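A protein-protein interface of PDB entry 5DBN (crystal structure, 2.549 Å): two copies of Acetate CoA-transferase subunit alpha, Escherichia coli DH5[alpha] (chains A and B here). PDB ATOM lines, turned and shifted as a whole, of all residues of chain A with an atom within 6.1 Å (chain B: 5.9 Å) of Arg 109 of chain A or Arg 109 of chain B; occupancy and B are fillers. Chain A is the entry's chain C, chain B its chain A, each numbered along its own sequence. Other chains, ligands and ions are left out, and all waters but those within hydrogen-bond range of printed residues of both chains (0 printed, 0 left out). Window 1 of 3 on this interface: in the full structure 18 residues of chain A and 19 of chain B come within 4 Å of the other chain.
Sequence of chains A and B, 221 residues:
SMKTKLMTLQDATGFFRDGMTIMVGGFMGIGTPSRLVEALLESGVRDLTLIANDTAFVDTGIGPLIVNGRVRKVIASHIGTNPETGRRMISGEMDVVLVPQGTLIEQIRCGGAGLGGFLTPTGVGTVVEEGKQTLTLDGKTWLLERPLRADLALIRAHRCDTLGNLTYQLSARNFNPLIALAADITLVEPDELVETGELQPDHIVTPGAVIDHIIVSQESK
Of the 15 printed residues of chain A, 2 touch a printed residue of chain B. Printed residues of chain B that touch a printed residue of chain A: Glu 106, Arg 109 and Leu 115. Hydrophobic or aromatic side chains of chain B within 4 Å of the printed part of chain A: Leu 115. Among the printed residues, 4 pairs touch across the chains. Among the printed residues, Asp or Glu carboxylates within 4 Å of a Lys or Arg side-chain nitrogen of the other chain: Glu 106 of chain A with Arg 109 of chain B and Arg 109 of chain A with Glu 106 of chain B.
The side-chain sulfur of Cys 110 of chain B lies close to the backbone carbonyl oxygen of Glu 106 of chain B (3.5 Å). The backbone carbonyl oxygen (O) of Glu 106 of chain A sits close to the side-chain sulfur (SG) of Cys 110 of chain A, at 3.5 Å. The backbone carbonyl oxygen of Cys 110 of chain B is in hydrogen-bond range of the backbone NH of Leu 115 of chain B.
Among the printed residues, pairs that only touch across the chains: Glu 106 of chain A with Leu 115 of chain B (3.8 Å).
Glu 106 of chain A touches Arg 109 of chain B, and with the chains exchanged Arg 109 of chain A touches Glu 106 of chain B. Glu 106 of chain A touches Leu 115 of chain B, but with the chains exchanged Leu 115 of chain A does not touch Glu 106 of chain B (4.01 Å). Arg 109 of chain A touches its own counterpart, Arg 109 of chain B. 15 positions are printed for both chains. Of the 4 pairs that touch across the chains among the printed residues, 3 have their exchanged pair printed and touching as well.
Arg 109 of chain A touches two residues of chain B. Of chain A, only Glu 106 (2.8 Å) and Arg 109 (3.1 Å) come within 4 Å of Arg 109 of chain B. Of the printed residues of chain B, Glu 106 of chain A touches Arg 109 (2.8 Å) and Leu 115 (3.8 Å). Of the printed residues of chain A, Leu 115 of chain B touches Glu 106. Gln 107 of chain B touches none of the printed residues of chain A. Leu 178 of chain B touches none of the printed residues of chain A. The nearest printed residue of chain A that does not touch Arg 109 of chain B is Leu 115 of chain A (6.5 Å). The nearest printed residue of chain B that does not touch Glu 106 of chain A is Ala 113 of chain B (5.3 Å).
OE2 of Glu 106 of chain B is in salt-bridge range of NH2 of Arg 109 of chain A, 2.8 Å away. NH2 of Arg 109 of chain A sits close to NE of Arg 109 of chain B, 3.3 Å away. NH2 of Arg 109 of chain B is in salt-bridge range of OE2 of Glu 106 of chain A, 2.8 Å away.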
ATOM      1  N   LEU A 104     -25.273  20.007  31.587  1.00  0.00           N
ATOM      2  CA  LEU A 104     -24.256  20.719  32.350  1.00  0.00           C
ATOM      3  C   LEU A 104     -22.930  19.962  32.360  1.00  0.00           C
ATOM      4  O   LEU A 104     -21.878  20.545  32.095  1.00  0.00           O
ATOM      5  CB  LEU A 104     -24.743  20.957  33.781  1.00  0.00           C
ATOM      6  CG  LEU A 104     -23.808  21.746  34.701  1.00  0.00           C
ATOM      7  CD1 LEU A 104     -23.551  23.152  34.179  1.00  0.00           C
ATOM      8  CD2 LEU A 104     -24.414  21.806  36.095  1.00  0.00           C
ATOM      9  N   ILE A 105     -22.977  18.674  32.681  1.00  0.00           N
ATOM     10  CA  ILE A 105     -21.762  17.870  32.739  1.00  0.00           C
ATOM     11  C   ILE A 105     -21.090  17.780  31.363  1.00  0.00           C
ATOM     12  O   ILE A 105     -19.864  17.752  31.267  1.00  0.00           O
ATOM     13  CB  ILE A 105     -22.046  16.449  33.292  1.00  0.00           C
ATOM     14  CG1 ILE A 105     -20.737  15.730  33.633  1.00  0.00           C
ATOM     15  CG2 ILE A 105     -22.885  15.623  32.318  1.00  0.00           C
ATOM     16  CD1 ILE A 105     -19.963  16.370  34.776  1.00  0.00           C
ATOM     17  N   GLU A 106     -21.891  17.737  30.301  1.00  0.00           N
ATOM     18  CA  GLU A 106     -21.343  17.701  28.946  1.00  0.00           C
ATOM     19  C   GLU A 106     -20.742  19.047  28.549  1.00  0.00           C
ATOM     20  O   GLU A 106     -19.778  19.100  27.786  1.00  0.00           O
ATOM     21  CB  GLU A 106     -22.416  17.292  27.934  1.00  0.00           C
ATOM     22  CG  GLU A 106     -22.631  15.793  27.828  1.00  0.00           C
ATOM     23  CD  GLU A 106     -21.384  15.056  27.368  1.00  0.00           C
ATOM     24  OE1 GLU A 106     -20.643  15.605  26.524  1.00  0.00           O
ATOM     25  OE2 GLU A 106     -21.138  13.934  27.857  1.00  0.00           O
ATOM     26  N   GLN A 107     -21.323  20.135  29.047  1.00  0.00           N
ATOM     27  CA  GLN A 107     -20.750  21.457  28.830  1.00  0.00           C
ATOM     28  C   GLN A 107     -19.370  21.530  29.480  1.00  0.00           C
ATOM     29  O   GLN A 107     -18.410  22.005  28.871  1.00  0.00           O
ATOM     30  CB  GLN A 107     -21.661  22.555  29.389  1.00  0.00           C
ATOM     31  CG  GLN A 107     -22.933  22.783  28.594  1.00  0.00           C
ATOM     32  CD  GLN A 107     -23.729  23.972  29.100  1.00  0.00           C
ATOM     33  OE1 GLN A 107     -24.594  23.832  29.965  1.00  0.00           O
ATOM     34  NE2 GLN A 107     -23.441  25.150  28.559  1.00  0.00           N
ATOM     35  N   ILE A 108     -19.287  21.058  30.722  1.00  0.00           N
ATOM     36  CA  ILE A 108     -18.019  20.998  31.446  1.00  0.00           C
ATOM     37  C   ILE A 108     -17.021  20.116  30.703  1.00  0.00           C
ATOM     38  O   ILE A 108     -15.856  20.482  30.561  1.00  0.00           O
ATOM     39  CB  ILE A 108     -18.203  20.478  32.889  1.00  0.00           C
ATOM     40  CG1 ILE A 108     -19.089  21.437  33.689  1.00  0.00           C
ATOM     41  CG2 ILE A 108     -16.851  20.339  33.595  1.00  0.00           C
ATOM     42  CD1 ILE A 108     -19.535  20.893  35.031  1.00  0.00           C
ATOM     43  N   ARG A 109     -17.467  18.940  30.265  1.00  0.00           N
ATOM     44  CA  ARG A 109     -16.604  18.034  29.509  1.00  0.00           C
ATOM     45  C   ARG A 109     -16.084  18.694  28.234  1.00  0.00           C
ATOM     46  O   ARG A 109     -14.904  18.566  27.901  1.00  0.00           O
ATOM     47  CB  ARG A 109     -17.338  16.738  29.154  1.00  0.00           C
ATOM     48  CG  ARG A 109     -16.449  15.731  28.432  1.00  0.00           C
ATOM     49  CD  ARG A 109     -17.178  14.448  28.079  1.00  0.00           C
ATOM     50  NE  ARG A 109     -16.284  13.501  27.414  1.00  0.00           N
ATOM     51  CZ  ARG A 109     -15.989  13.523  26.115  1.00  0.00           C
ATOM     52  NH1 ARG A 109     -16.525  14.437  25.316  1.00  0.00           N
ATOM     53  NH2 ARG A 109     -15.158  12.621  25.610  1.00  0.00           N
ATOM     54  N   CYS A 110     -16.966  19.390  27.522  1.00  0.00           N
ATOM     55  CA  CYS A 110     -16.573  20.109  26.313  1.00  0.00           C
ATOM     56  C   CYS A 110     -15.510  21.151  26.634  1.00  0.00           C
ATOM     57  O   CYS A 110     -14.515  21.277  25.919  1.00  0.00           O
ATOM     58  CB  CYS A 110     -17.782  20.783  25.658  1.00  0.00           C
ATOM     59  SG  CYS A 110     -18.694  19.736  24.510  1.00  0.00           S
ATOM     60  N   GLY A 111     -15.739  21.906  27.703  1.00  0.00           N
ATOM     61  CA  GLY A 111     -14.778  22.886  28.172  1.00  0.00           C
ATOM     62  C   GLY A 111     -13.421  22.270  28.455  1.00  0.00           C
ATOM     63  O   GLY A 111     -12.380  22.856  28.158  1.00  0.00           O
ATOM     64  N   GLY A 112     -13.438  21.078  29.041  1.00  0.00           N
ATOM     65  CA  GLY A 112     -12.218  20.370  29.367  1.00  0.00           C
ATOM     66  C   GLY A 112     -11.573  19.659  28.193  1.00  0.00           C
ATOM     67  O   GLY A 112     -10.354  19.463  28.179  1.00  0.00           O
ATOM     68  N   ALA A 113     -12.389  19.259  27.221  1.00  0.00           N
ATOM     69  CA  ALA A 113     -11.918  18.435  26.110  1.00  0.00           C
ATOM     70  C   ALA A 113     -11.666  19.244  24.845  1.00  0.00           C
ATOM     71  O   ALA A 113     -11.393  18.676  23.784  1.00  0.00           O
ATOM     72  CB  ALA A 113     -12.922  17.323  25.825  1.00  0.00           C
ATOM     73  N   GLY A 114     -11.756  20.565  24.953  1.00  0.00           N
ATOM     74  CA  GLY A 114     -11.466  21.436  23.828  1.00  0.00           C
ATOM     75  C   GLY A 114     -12.467  21.326  22.691  1.00  0.00           C
ATOM     76  O   GLY A 114     -12.109  21.491  21.524  1.00  0.00           O
ATOM     77  N   LEU A 115     -13.721  21.044  23.031  1.00  0.00           N
ATOM     78  CA  LEU A 115     -14.790  20.967  22.041  1.00  0.00           C
ATOM     79  C   LEU A 115     -15.590  22.268  22.039  1.00  0.00           C
ATOM     80  O   LEU A 115     -15.756  22.906  23.080  1.00  0.00           O
ATOM     81  CB  LEU A 115     -15.701  19.775  22.334  1.00  0.00           C
ATOM     82  CG  LEU A 115     -15.014  18.408  22.274  1.00  0.00           C
ATOM     83  CD1 LEU A 115     -15.938  17.329  22.806  1.00  0.00           C
ATOM     84  CD2 LEU A 115     -14.573  18.079  20.853  1.00  0.00           C
ATOM     85  N   LEU A 148     -18.311  25.023  28.996  1.00  0.00           N
ATOM     86  CA  LEU A 148     -18.118  25.820  30.202  1.00  0.00           C
ATOM     87  C   LEU A 148     -16.718  25.596  30.772  1.00  0.00           C
ATOM     88  O   LEU A 148     -16.266  24.458  30.905  1.00  0.00           O
ATOM     89  CB  LEU A 148     -19.175  25.473  31.252  1.00  0.00           C
ATOM     90  CG  LEU A 148     -20.574  26.058  31.053  1.00  0.00           C
ATOM     91  CD1 LEU A 148     -21.553  25.446  32.049  1.00  0.00           C
ATOM     92  CD2 LEU A 148     -20.561  27.572  31.185  1.00  0.00           C
ATOM     93  N   LEU A 178     -14.336  15.647  35.835  1.00  0.00           N
ATOM     94  CA  LEU A 178     -14.576  16.504  34.675  1.00  0.00           C
ATOM     95  C   LEU A 178     -14.092  17.938  34.895  1.00  0.00           C
ATOM     96  O   LEU A 178     -13.479  18.527  34.008  1.00  0.00           O
ATOM     97  CB  LEU A 178     -16.067  16.518  34.320  1.00  0.00           C
ATOM     98  CG  LEU A 178     -16.681  15.260  33.693  1.00  0.00           C
ATOM     99  CD1 LEU A 178     -15.911  14.821  32.452  1.00  0.00           C
ATOM    100  CD2 LEU A 178     -16.782  14.116  34.699  1.00  0.00           C
ATOM    101  N   ALA A 182     -11.385  21.173  33.070  1.00  0.00           N
ATOM    102  CA  ALA A 182     -12.079  22.345  32.536  1.00  0.00           C
ATOM    103  C   ALA A 182     -11.656  23.667  33.176  1.00  0.00           C
ATOM    104  O   ALA A 182     -12.195  24.720  32.831  1.00  0.00           O
ATOM    105  CB  ALA A 182     -13.584  22.164  32.691  1.00  0.00           C
ATOM    106  N   LEU B 104     -12.794  10.599  15.356  1.00  0.00           N
ATOM    107  CA  LEU B 104     -13.395   9.273  15.242  1.00  0.00           C
ATOM    108  C   LEU B 104     -13.903   8.759  16.586  1.00  0.00           C
ATOM    109  O   LEU B 104     -15.046   8.319  16.694  1.00  0.00           O
ATOM    110  CB  LEU B 104     -12.384   8.279  14.663  1.00  0.00           C
ATOM    111  CG  LEU B 104     -12.900   6.857  14.425  1.00  0.00           C
ATOM    112  CD1 LEU B 104     -14.026   6.823  13.399  1.00  0.00           C
ATOM    113  CD2 LEU B 104     -11.749   5.953  14.004  1.00  0.00           C
ATOM    114  N   ILE B 105     -13.049   8.805  17.601  1.00  0.00           N
ATOM    115  CA  ILE B 105     -13.420   8.316  18.924  1.00  0.00           C
ATOM    116  C   ILE B 105     -14.576   9.129  19.508  1.00  0.00           C
ATOM    117  O   ILE B 105     -15.433   8.587  20.202  1.00  0.00           O
ATOM    118  CB  ILE B 105     -12.212   8.332  19.899  1.00  0.00           C
ATOM    119  CG1 ILE B 105     -12.537   7.557  21.179  1.00  0.00           C
ATOM    120  CG2 ILE B 105     -11.785   9.757  20.237  1.00  0.00           C
ATOM    121  CD1 ILE B 105     -12.758   6.062  20.968  1.00  0.00           C
ATOM    122  N   GLU B 106     -14.598  10.425  19.221  1.00  0.00           N
ATOM    123  CA  GLU B 106     -15.675  11.291  19.693  1.00  0.00           C
ATOM    124  C   GLU B 106     -16.979  11.019  18.942  1.00  0.00           C
ATOM    125  O   GLU B 106     -18.066  11.142  19.511  1.00  0.00           O
ATOM    126  CB  GLU B 106     -15.282  12.763  19.547  1.00  0.00           C
ATOM    127  CG  GLU B 106     -14.383  13.274  20.661  1.00  0.00           C
ATOM    128  CD  GLU B 106     -15.026  13.177  22.033  1.00  0.00           C
ATOM    129  OE1 GLU B 106     -16.253  13.392  22.138  1.00  0.00           O
ATOM    130  OE2 GLU B 106     -14.303  12.871  23.004  1.00  0.00           O
ATOM    131  N   GLN B 107     -16.871  10.658  17.665  1.00  0.00           N
ATOM    132  CA  GLN B 107     -18.040  10.253  16.889  1.00  0.00           C
ATOM    133  C   GLN B 107     -18.652   9.000  17.499  1.00  0.00           C
ATOM    134  O   GLN B 107     -19.872   8.891  17.629  1.00  0.00           O
ATOM    135  CB  GLN B 107     -17.683  10.000  15.424  1.00  0.00           C
ATOM    136  CG  GLN B 107     -17.382  11.245  14.612  1.00  0.00           C
ATOM    137  CD  GLN B 107     -17.174  10.931  13.142  1.00  0.00           C
ATOM    138  OE1 GLN B 107     -16.053  10.675  12.703  1.00  0.00           O
ATOM    139  NE2 GLN B 107     -18.262  10.936  12.374  1.00  0.00           N
ATOM    140  N   ILE B 108     -17.792   8.043  17.836  1.00  0.00           N
ATOM    141  CA  ILE B 108     -18.218   6.819  18.500  1.00  0.00           C
ATOM    142  C   ILE B 108     -18.870   7.132  19.846  1.00  0.00           C
ATOM    143  O   ILE B 108     -19.948   6.619  20.152  1.00  0.00           O
ATOM    144  CB  ILE B 108     -17.036   5.850  18.711  1.00  0.00           C
ATOM    145  CG1 ILE B 108     -16.453   5.422  17.363  1.00  0.00           C
ATOM    146  CG2 ILE B 108     -17.481   4.614  19.491  1.00  0.00           C
ATOM    147  CD1 ILE B 108     -15.135   4.679  17.465  1.00  0.00           C
ATOM    148  N   ARG B 109     -18.211   7.962  20.651  1.00  0.00           N
ATOM    149  CA  ARG B 109     -18.760   8.345  21.946  1.00  0.00           C
ATOM    150  C   ARG B 109     -20.115   9.030  21.806  1.00  0.00           C
ATOM    151  O   ARG B 109     -21.035   8.744  22.570  1.00  0.00           O
ATOM    152  CB  ARG B 109     -17.804   9.266  22.703  1.00  0.00           C
ATOM    153  CG  ARG B 109     -18.317   9.621  24.094  1.00  0.00           C
ATOM    154  CD  ARG B 109     -17.387  10.546  24.841  1.00  0.00           C
ATOM    155  NE  ARG B 109     -17.909  10.838  26.174  1.00  0.00           N
ATOM    156  CZ  ARG B 109     -18.828  11.761  26.439  1.00  0.00           C
ATOM    157  NH1 ARG B 109     -19.338  12.502  25.463  1.00  0.00           N
ATOM    158  NH2 ARG B 109     -19.237  11.947  27.687  1.00  0.00           N
ATOM    159  N   CYS B 110     -20.229   9.941  20.844  1.00  0.00           N
ATOM    160  CA  CYS B 110     -21.493  10.626  20.592  1.00  0.00           C
ATOM    161  C   CYS B 110     -22.588   9.629  20.244  1.00  0.00           C
ATOM    162  O   CYS B 110     -23.699   9.705  20.769  1.00  0.00           O
ATOM    163  CB  CYS B 110     -21.344  11.655  19.469  1.00  0.00           C
ATOM    164  SG  CYS B 110     -20.798  13.277  20.032  1.00  0.00           S
ATOM    165  N   GLY B 111     -22.263   8.698  19.353  1.00  0.00           N
ATOM    166  CA  GLY B 111     -23.170   7.623  18.998  1.00  0.00           C
ATOM    167  C   GLY B 111     -23.603   6.848  20.228  1.00  0.00           C
ATOM    168  O   GLY B 111     -24.751   6.422  20.341  1.00  0.00           O
ATOM    169  N   GLY B 112     -22.662   6.651  21.144  1.00  0.00           N
ATOM    170  CA  GLY B 112     -22.923   5.931  22.375  1.00  0.00           C
ATOM    171  C   GLY B 112     -23.623   6.725  23.463  1.00  0.00           C
ATOM    172  O   GLY B 112     -24.333   6.150  24.290  1.00  0.00           O
ATOM    173  N   ALA B 113     -23.421   8.038  23.473  1.00  0.00           N
ATOM    174  CA  ALA B 113     -23.925   8.883  24.555  1.00  0.00           C
ATOM    175  C   ALA B 113     -25.218   9.598  24.180  1.00  0.00           C
ATOM    176  O   ALA B 113     -25.698  10.451  24.926  1.00  0.00           O
ATOM    177  CB  ALA B 113     -22.866   9.897  24.958  1.00  0.00           C
ATOM    178  N   GLY B 114     -25.784   9.246  23.031  1.00  0.00           N
ATOM    179  CA  GLY B 114     -27.047   9.815  22.596  1.00  0.00           C
ATOM    180  C   GLY B 114     -26.979  11.293  22.241  1.00  0.00           C
ATOM    181  O   GLY B 114     -27.955  12.023  22.413  1.00  0.00           O
ATOM    182  N   LEU B 115     -25.826  11.731  21.744  1.00  0.00           N
ATOM    183  CA  LEU B 115     -25.651  13.109  21.297  1.00  0.00           C
ATOM    184  C   LEU B 115     -25.763  13.176  19.779  1.00  0.00           C
ATOM    185  O   LEU B 115     -25.413  12.225  19.081  1.00  0.00           O
ATOM    186  CB  LEU B 115     -24.304  13.665  21.766  1.00  0.00           C
ATOM    187  CG  LEU B 115     -24.122  13.741  23.286  1.00  0.00           C
ATOM    188  CD1 LEU B 115     -22.685  14.090  23.640  1.00  0.00           C
ATOM    189  CD2 LEU B 115     -25.077  14.753  23.898  1.00  0.00           C
ATOM    190  N   LEU B 148     -21.421   8.151  15.267  1.00  0.00           N
ATOM    191  CA  LEU B 148     -21.248   6.864  14.595  1.00  0.00           C
ATOM    192  C   LEU B 148     -21.776   5.734  15.463  1.00  0.00           C
ATOM    193  O   LEU B 148     -21.451   5.648  16.650  1.00  0.00           O
ATOM    194  CB  LEU B 148     -19.774   6.593  14.278  1.00  0.00           C
ATOM    195  CG  LEU B 148     -19.124   7.279  13.079  1.00  0.00           C
ATOM    196  CD1 LEU B 148     -17.625   7.019  13.113  1.00  0.00           C
ATOM    197  CD2 LEU B 148     -19.725   6.796  11.767  1.00  0.00           C
ATOM    198  N   LEU B 178     -15.561   2.690  24.585  1.00  0.00           N
ATOM    199  CA  LEU B 178     -16.456   3.575  23.846  1.00  0.00           C
ATOM    200  C   LEU B 178     -17.361   2.810  22.884  1.00  0.00           C
ATOM    201  O   LEU B 178     -18.558   3.084  22.806  1.00  0.00           O
ATOM    202  CB  LEU B 178     -15.656   4.624  23.069  1.00  0.00           C
ATOM    203  CG  LEU B 178     -14.970   5.745  23.860  1.00  0.00           C
ATOM    204  CD1 LEU B 178     -15.962   6.485  24.748  1.00  0.00           C
ATOM    205  CD2 LEU B 178     -13.803   5.218  24.682  1.00  0.00           C
ATOM    206  N   ALA B 182     -21.692   2.254  21.819  1.00  0.00           N
ATOM    207  CA  ALA B 182     -22.082   2.780  20.512  1.00  0.00           C
ATOM    208  C   ALA B 182     -22.680   1.729  19.576  1.00  0.00           C
ATOM    209  O   ALA B 182     -23.064   2.052  18.450  1.00  0.00           O
ATOM    210  CB  ALA B 182     -20.877   3.425  19.848  1.00  0.00           C
